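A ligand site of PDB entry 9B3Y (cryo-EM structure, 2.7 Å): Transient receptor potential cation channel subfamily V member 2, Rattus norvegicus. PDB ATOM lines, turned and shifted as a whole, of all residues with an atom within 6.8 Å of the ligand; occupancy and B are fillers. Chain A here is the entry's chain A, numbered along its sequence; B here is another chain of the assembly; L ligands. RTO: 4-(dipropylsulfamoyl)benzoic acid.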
ATOM      1  N   GLU A 113      32.177 -25.722 -25.061  1.00  0.00           N
ATOM      2  CA  GLU A 113      32.058 -26.839 -24.115  1.00  0.00           C
ATOM      3  C   GLU A 113      31.790 -28.182 -24.830  1.00  0.00           C
ATOM      4  O   GLU A 113      31.227 -28.224 -25.927  1.00  0.00           O
ATOM      5  CB  GLU A 113      30.992 -26.538 -23.034  1.00  0.00           C
ATOM      6  CG  GLU A 113      31.355 -27.126 -21.680  1.00  0.00           C
ATOM      7  CD  GLU A 113      30.555 -26.546 -20.509  1.00  0.00           C
ATOM      8  OE1 GLU A 113      29.333 -26.779 -20.427  1.00  0.00           O
ATOM      9  OE2 GLU A 113      31.140 -25.865 -19.648  1.00  0.00           O
ATOM     10  N   THR A 116      28.447 -30.265 -27.147  1.00  0.00           N
ATOM     11  CA  THR A 116      27.483 -29.186 -27.451  1.00  0.00           C
ATOM     12  C   THR A 116      28.175 -28.068 -28.254  1.00  0.00           C
ATOM     13  O   THR A 116      29.267 -28.263 -28.778  1.00  0.00           O
ATOM     14  CB  THR A 116      26.827 -28.698 -26.141  1.00  0.00           C
ATOM     15  OG1 THR A 116      25.797 -27.780 -26.420  1.00  0.00           O
ATOM     16  CG2 THR A 116      27.773 -28.035 -25.157  1.00  0.00           C
ATOM     17  N   LYS A 118      28.122 -24.729 -26.771  1.00  0.00           N
ATOM     18  CA  LYS A 118      28.033 -23.722 -25.704  1.00  0.00           C
ATOM     19  C   LYS A 118      29.315 -22.889 -25.592  1.00  0.00           C
ATOM     20  O   LYS A 118      30.387 -23.442 -25.380  1.00  0.00           O
ATOM     21  CB  LYS A 118      27.721 -24.501 -24.433  1.00  0.00           C
ATOM     22  CG  LYS A 118      27.530 -23.702 -23.145  1.00  0.00           C
ATOM     23  CD  LYS A 118      27.120 -24.719 -22.067  1.00  0.00           C
ATOM     24  CE  LYS A 118      27.141 -24.160 -20.651  1.00  0.00           C
ATOM     25  NZ  LYS A 118      27.081 -25.278 -19.672  1.00  0.00           N
ATOM     26  N   MET A 122      27.854 -17.842 -23.109  1.00  0.00           N
ATOM     27  CA  MET A 122      26.880 -18.612 -22.325  1.00  0.00           C
ATOM     28  C   MET A 122      27.432 -18.912 -20.919  1.00  0.00           C
ATOM     29  O   MET A 122      26.732 -18.699 -19.929  1.00  0.00           O
ATOM     30  CB  MET A 122      26.502 -19.882 -23.093  1.00  0.00           C
ATOM     31  CG  MET A 122      25.880 -19.527 -24.441  1.00  0.00           C
ATOM     32  SD  MET A 122      25.391 -20.955 -25.417  1.00  0.00           S
ATOM     33  CE  MET A 122      25.487 -20.236 -27.072  1.00  0.00           C
ATOM     34  N   LEU A 126      25.533 -17.517 -17.537  1.00  0.00           N
ATOM     35  CA  LEU A 126      25.171 -18.448 -16.471  1.00  0.00           C
ATOM     36  C   LEU A 126      25.676 -18.040 -15.067  1.00  0.00           C
ATOM     37  O   LEU A 126      25.210 -18.570 -14.063  1.00  0.00           O
ATOM     38  CB  LEU A 126      25.683 -19.859 -16.846  1.00  0.00           C
ATOM     39  CG  LEU A 126      24.869 -20.523 -17.964  1.00  0.00           C
ATOM     40  CD1 LEU A 126      25.650 -21.670 -18.595  1.00  0.00           C
ATOM     41  CD2 LEU A 126      23.561 -21.082 -17.447  1.00  0.00           C
ATOM     42  N   ASN A 127      26.617 -17.092 -14.980  1.00  0.00           N
ATOM     43  CA  ASN A 127      27.326 -16.688 -13.759  1.00  0.00           C
ATOM     44  C   ASN A 127      27.122 -15.199 -13.428  1.00  0.00           C
ATOM     45  O   ASN A 127      28.065 -14.496 -13.065  1.00  0.00           O
ATOM     46  CB  ASN A 127      28.795 -17.132 -13.876  1.00  0.00           C
ATOM     47  CG  ASN A 127      28.946 -18.633 -13.743  1.00  0.00           C
ATOM     48  OD1 ASN A 127      28.814 -19.198 -12.672  1.00  0.00           O
ATOM     49  ND2 ASN A 127      29.212 -19.340 -14.814  1.00  0.00           N
ATOM     50  N   CYS A 157      23.999 -23.249 -29.328  1.00  0.00           N
ATOM     51  CA  CYS A 157      24.246 -24.670 -29.146  1.00  0.00           C
ATOM     52  C   CYS A 157      23.797 -25.483 -30.376  1.00  0.00           C
ATOM     53  O   CYS A 157      22.903 -25.051 -31.113  1.00  0.00           O
ATOM     54  CB  CYS A 157      23.560 -25.121 -27.856  1.00  0.00           C
ATOM     55  SG  CYS A 157      24.246 -24.215 -26.445  1.00  0.00           S
ATOM     56  N   PHE A 161      19.732 -32.005 -28.426  1.00  0.00           N
ATOM     57  CA  PHE A 161      18.887 -31.554 -27.324  1.00  0.00           C
ATOM     58  C   PHE A 161      18.825 -30.039 -27.226  1.00  0.00           C
ATOM     59  O   PHE A 161      17.725 -29.501 -27.138  1.00  0.00           O
ATOM     60  CB  PHE A 161      19.337 -32.177 -26.007  1.00  0.00           C
ATOM     61  CG  PHE A 161      18.873 -33.599 -25.858  1.00  0.00           C
ATOM     62  CD1 PHE A 161      17.570 -33.860 -25.400  1.00  0.00           C
ATOM     63  CD2 PHE A 161      19.722 -34.673 -26.170  1.00  0.00           C
ATOM     64  CE1 PHE A 161      17.119 -35.172 -25.261  1.00  0.00           C
ATOM     65  CE2 PHE A 161      19.273 -35.999 -26.022  1.00  0.00           C
ATOM     66  CZ  PHE A 161      17.974 -36.252 -25.561  1.00  0.00           C
ATOM     67  N   TYR A 162      19.952 -29.336 -27.281  1.00  0.00           N
ATOM     68  CA  TYR A 162      19.991 -27.883 -27.046  1.00  0.00           C
ATOM     69  C   TYR A 162      20.127 -27.041 -28.321  1.00  0.00           C
ATOM     70  O   TYR A 162      20.381 -25.845 -28.229  1.00  0.00           O
ATOM     71  CB  TYR A 162      21.043 -27.536 -25.985  1.00  0.00           C
ATOM     72  CG  TYR A 162      20.876 -28.352 -24.717  1.00  0.00           C
ATOM     73  CD1 TYR A 162      19.762 -28.133 -23.884  1.00  0.00           C
ATOM     74  CD2 TYR A 162      21.784 -29.376 -24.405  1.00  0.00           C
ATOM     75  CE1 TYR A 162      19.531 -28.962 -22.774  1.00  0.00           C
ATOM     76  CE2 TYR A 162      21.548 -30.214 -23.297  1.00  0.00           C
ATOM     77  CZ  TYR A 162      20.409 -30.019 -22.499  1.00  0.00           C
ATOM     78  OH  TYR A 162      20.150 -30.858 -21.465  1.00  0.00           O
ATOM     79  N   HIS A 165      19.730 -22.945 -28.861  1.00  0.00           N
ATOM     80  CA  HIS A 165      19.834 -22.255 -27.576  1.00  0.00           C
ATOM     81  C   HIS A 165      20.943 -21.204 -27.604  1.00  0.00           C
ATOM     82  O   HIS A 165      22.017 -21.465 -28.145  1.00  0.00           O
ATOM     83  CB  HIS A 165      20.101 -23.274 -26.478  1.00  0.00           C
ATOM     84  CG  HIS A 165      20.143 -22.692 -25.094  1.00  0.00           C
ATOM     85  ND1 HIS A 165      19.188 -21.835 -24.564  1.00  0.00           N
ATOM     86  CD2 HIS A 165      21.043 -23.020 -24.122  1.00  0.00           C
ATOM     87  CE1 HIS A 165      19.545 -21.639 -23.294  1.00  0.00           C
ATOM     88  NE2 HIS A 165      20.647 -22.333 -22.995  1.00  0.00           N
ATOM     89  N   ILE A 170      19.418 -17.708 -22.232  1.00  0.00           N
ATOM     90  CA  ILE A 170      19.953 -17.840 -20.870  1.00  0.00           C
ATOM     91  C   ILE A 170      19.657 -16.574 -20.068  1.00  0.00           C
ATOM     92  O   ILE A 170      19.139 -16.657 -18.948  1.00  0.00           O
ATOM     93  CB  ILE A 170      21.462 -18.173 -20.857  1.00  0.00           C
ATOM     94  CG1 ILE A 170      21.753 -19.464 -21.643  1.00  0.00           C
ATOM     95  CG2 ILE A 170      21.966 -18.340 -19.415  1.00  0.00           C
ATOM     96  CD1 ILE A 170      23.235 -19.767 -21.798  1.00  0.00           C
ATOM     97  N   GLU A 173      15.910 -16.520 -19.095  1.00  0.00           N
ATOM     98  CA  GLU A 173      15.550 -17.510 -18.059  1.00  0.00           C
ATOM     99  C   GLU A 173      16.135 -17.169 -16.689  1.00  0.00           C
ATOM    100  O   GLU A 173      15.443 -17.301 -15.687  1.00  0.00           O
ATOM    101  CB  GLU A 173      15.956 -18.921 -18.507  1.00  0.00           C
ATOM    102  CG  GLU A 173      15.447 -20.018 -17.544  1.00  0.00           C
ATOM    103  CD  GLU A 173      16.307 -20.260 -16.292  1.00  0.00           C
ATOM    104  OE1 GLU A 173      17.516 -19.944 -16.269  1.00  0.00           O
ATOM    105  OE2 GLU A 173      15.765 -20.841 -15.314  1.00  0.00           O
ATOM    106  N   LYS A 174      17.365 -16.641 -16.646  1.00  0.00           N
ATOM    107  CA  LYS A 174      18.005 -16.081 -15.437  1.00  0.00           C
ATOM    108  C   LYS A 174      17.377 -14.753 -14.968  1.00  0.00           C
ATOM    109  O   LYS A 174      17.829 -14.185 -13.970  1.00  0.00           O
ATOM    110  CB  LYS A 174      19.519 -15.955 -15.706  1.00  0.00           C
ATOM    111  CG  LYS A 174      20.224 -17.313 -15.859  1.00  0.00           C
ATOM    112  CD  LYS A 174      20.407 -18.036 -14.520  1.00  0.00           C
ATOM    113  CE  LYS A 174      20.874 -19.489 -14.702  1.00  0.00           C
ATOM    114  NZ  LYS A 174      19.742 -20.448 -14.755  1.00  0.00           N
ATOM    115  N   PHE A 198      15.210 -30.645 -26.297  1.00  0.00           N
ATOM    116  CA  PHE A 198      14.873 -30.188 -24.947  1.00  0.00           C
ATOM    117  C   PHE A 198      13.759 -29.133 -24.944  1.00  0.00           C
ATOM    118  O   PHE A 198      12.959 -29.063 -24.015  1.00  0.00           O
ATOM    119  CB  PHE A 198      16.142 -29.656 -24.293  1.00  0.00           C
ATOM    120  CG  PHE A 198      15.914 -29.084 -22.915  1.00  0.00           C
ATOM    121  CD1 PHE A 198      15.453 -29.900 -21.868  1.00  0.00           C
ATOM    122  CD2 PHE A 198      16.139 -27.719 -22.678  1.00  0.00           C
ATOM    123  CE1 PHE A 198      15.212 -29.354 -20.607  1.00  0.00           C
ATOM    124  CE2 PHE A 198      15.878 -27.166 -21.413  1.00  0.00           C
ATOM    125  CZ  PHE A 198      15.420 -27.980 -20.375  1.00  0.00           C
ATOM    126  N   PHE A 199      13.659 -28.323 -25.989  1.00  0.00           N
ATOM    127  CA  PHE A 199      12.703 -27.222 -26.124  1.00  0.00           C
ATOM    128  C   PHE A 199      11.430 -27.588 -26.872  1.00  0.00           C
ATOM    129  O   PHE A 199      10.504 -26.786 -26.957  1.00  0.00           O
ATOM    130  CB  PHE A 199      13.397 -26.074 -26.846  1.00  0.00           C
ATOM    131  CG  PHE A 199      14.706 -25.677 -26.209  1.00  0.00           C
ATOM    132  CD1 PHE A 199      14.720 -25.119 -24.925  1.00  0.00           C
ATOM    133  CD2 PHE A 199      15.907 -25.904 -26.880  1.00  0.00           C
ATOM    134  CE1 PHE A 199      15.927 -24.706 -24.346  1.00  0.00           C
ATOM    135  CE2 PHE A 199      17.114 -25.537 -26.298  1.00  0.00           C
ATOM    136  CZ  PHE A 199      17.123 -24.927 -25.029  1.00  0.00           C
ATOM    137  N   THR B 331      22.634 -30.045  -7.107  1.00  0.00           N
ATOM    138  CA  THR B 331      22.050 -29.497  -8.335  1.00  0.00           C
ATOM    139  C   THR B 331      23.151 -29.241  -9.368  1.00  0.00           C
ATOM    140  O   THR B 331      24.068 -28.471  -9.113  1.00  0.00           O
ATOM    141  CB  THR B 331      21.261 -28.203  -8.084  1.00  0.00           C
ATOM    142  OG1 THR B 331      20.226 -28.432  -7.151  1.00  0.00           O
ATOM    143  CG2 THR B 331      20.584 -27.703  -9.355  1.00  0.00           C
ATOM    144  N   GLU B 332      23.080 -29.884 -10.524  1.00  0.00           N
ATOM    145  CA  GLU B 332      24.029 -29.737 -11.622  1.00  0.00           C
ATOM    146  C   GLU B 332      23.727 -28.492 -12.459  1.00  0.00           C
ATOM    147  O   GLU B 332      24.603 -27.655 -12.685  1.00  0.00           O
ATOM    148  CB  GLU B 332      24.019 -31.003 -12.487  1.00  0.00           C
ATOM    149  CG  GLU B 332      25.035 -30.907 -13.620  1.00  0.00           C
ATOM    150  CD  GLU B 332      25.036 -32.130 -14.528  1.00  0.00           C
ATOM    151  OE1 GLU B 332      24.891 -33.272 -14.040  1.00  0.00           O
ATOM    152  OE2 GLU B 332      25.223 -31.965 -15.761  1.00  0.00           O
ATOM    153  N   TRP B 333      22.479 -28.356 -12.902  1.00  0.00           N
ATOM    154  CA  TRP B 333      21.948 -27.141 -13.527  1.00  0.00           C
ATOM    155  C   TRP B 333      20.449 -27.026 -13.290  1.00  0.00           C
ATOM    156  O   TRP B 333      19.749 -27.995 -13.018  1.00  0.00           O
ATOM    157  CB  TRP B 333      22.329 -27.065 -15.015  1.00  0.00           C
ATOM    158  CG  TRP B 333      21.843 -28.138 -15.943  1.00  0.00           C
ATOM    159  CD1 TRP B 333      22.607 -29.151 -16.408  1.00  0.00           C
ATOM    160  CD2 TRP B 333      20.545 -28.289 -16.591  1.00  0.00           C
ATOM    161  NE1 TRP B 333      21.873 -29.910 -17.294  1.00  0.00           N
ATOM    162  CE2 TRP B 333      20.607 -29.415 -17.460  1.00  0.00           C
ATOM    163  CE3 TRP B 333      19.321 -27.592 -16.557  1.00  0.00           C
ATOM    164  CZ2 TRP B 333      19.520 -29.824 -18.241  1.00  0.00           C
ATOM    165  CZ3 TRP B 333      18.215 -28.010 -17.325  1.00  0.00           C
ATOM    166  CH2 TRP B 333      18.317 -29.113 -18.175  1.00  0.00           C
ATOM    167  N   CYS B 334      19.944 -25.809 -13.419  1.00  0.00           N
ATOM    168  CA  CYS B 334      18.521 -25.482 -13.346  1.00  0.00           C
ATOM    169  C   CYS B 334      18.189 -24.486 -14.462  1.00  0.00           C
ATOM    170  O   CYS B 334      18.917 -23.515 -14.669  1.00  0.00           O
ATOM    171  CB  CYS B 334      18.223 -24.944 -11.947  1.00  0.00           C
ATOM    172  SG  CYS B 334      16.491 -24.477 -11.807  1.00  0.00           S
ATOM    173  N   TYR B 335      17.098 -24.732 -15.186  1.00  0.00           N
ATOM    174  CA  TYR B 335      16.661 -23.896 -16.302  1.00  0.00           C
ATOM    175  C   TYR B 335      15.150 -23.968 -16.456  1.00  0.00           C
ATOM    176  O   TYR B 335      14.590 -25.011 -16.813  1.00  0.00           O
ATOM    177  CB  TYR B 335      17.392 -24.311 -17.582  1.00  0.00           C
ATOM    178  CG  TYR B 335      17.171 -23.378 -18.751  1.00  0.00           C
ATOM    179  CD1 TYR B 335      17.990 -22.239 -18.897  1.00  0.00           C
ATOM    180  CD2 TYR B 335      16.140 -23.622 -19.669  1.00  0.00           C
ATOM    181  CE1 TYR B 335      17.749 -21.338 -19.938  1.00  0.00           C
ATOM    182  CE2 TYR B 335      15.915 -22.722 -20.726  1.00  0.00           C
ATOM    183  CZ  TYR B 335      16.701 -21.565 -20.849  1.00  0.00           C
ATOM    184  OH  TYR B 335      16.435 -20.682 -21.838  1.00  0.00           O
HETATM  185  C13 RTO L   1      21.587 -23.404 -15.722  1.00  0.00           C
HETATM  186  C15 RTO L   1      23.904 -24.061 -15.810  1.00  0.00           C
HETATM  187  C17 RTO L   1      22.854 -23.507 -13.623  1.00  0.00           C
HETATM  188  C01 RTO L   1      19.123 -25.510 -21.970  1.00  0.00           C
HETATM  189  C02 RTO L   1      19.541 -26.355 -20.766  1.00  0.00           C
HETATM  190  C03 RTO L   1      20.166 -25.443 -19.724  1.00  0.00           C
HETATM  191  C05 RTO L   1      22.281 -26.737 -19.599  1.00  0.00           C
HETATM  192  C06 RTO L   1      22.919 -27.286 -20.872  1.00  0.00           C
HETATM  193  C07 RTO L   1      23.482 -28.666 -20.552  1.00  0.00           C
HETATM  194  C11 RTO L   1      22.607 -23.933 -17.808  1.00  0.00           C
HETATM  195  C12 RTO L   1      21.508 -23.525 -17.091  1.00  0.00           C
HETATM  196  C14 RTO L   1      22.785 -23.661 -15.080  1.00  0.00           C
HETATM  197  C16 RTO L   1      23.808 -24.188 -17.175  1.00  0.00           C
HETATM  198  N04 RTO L   1      21.623 -25.469 -19.865  1.00  0.00           N
HETATM  199  O09 RTO L   1      21.548 -23.028 -19.864  1.00  0.00           O
HETATM  200  O10 RTO L   1      23.729 -24.178 -20.103  1.00  0.00           O
HETATM  201  O18 RTO L   1      21.859 -23.203 -13.002  1.00  0.00           O
HETATM  202  O19 RTO L   1      24.011 -23.703 -12.975  1.00  0.00           O
HETATM  203  S08 RTO L   1      22.432 -24.069 -19.541  1.00  0.00           S
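N of Cys 334 of chain B is in hydrogen-bond range of O18 of the ligand (3.3 Å).
A ring nitrogen (NE2) of His 165 sits at hydrogen-bond distance from an oxygen (O09) of the ligand (3.3 Å).
The side-chain amino group of Lys 174 is in salt-bridge range of an oxygen (O18) of the ligand (3.9 Å).
Residues that only touch the ligand: Leu 126, Tyr 162, Trp 333 of chain B, Lys 118, Tyr 335 of chain B, Phe 198, Phe 199 and Ile 170.
Hydrophobic or aromatic side chains within 4 Å of the ligand: Leu 126, Tyr 162, His 165, Ile 170, Phe 198, Phe 199, Trp 333 of chain B and Tyr 335 of chain B.
Of the 20 residues printed, 11 come within 4 Å of the ligand.
O of Cys 334 of chain B lies within hydrogen-bond range of NZ of Lys 174 (3.2 Å).
The backbone NH of Cys 157 lies within hydrogen-bond range of the backbone carbonyl oxygen of His 165, 2.9 Å away.
The side-chain amino group (NZ) of Lys 118 lies within salt-bridge range of the side-chain carboxylate (OE1) of Glu 113.
The side-chain amino group (NZ) of Lys 174 lies within salt-bridge range of the side-chain carboxylate (OE1) of Glu 173.
N of Phe 198 is in hydrogen-bond range of O of Phe 161 (2.9 Å).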
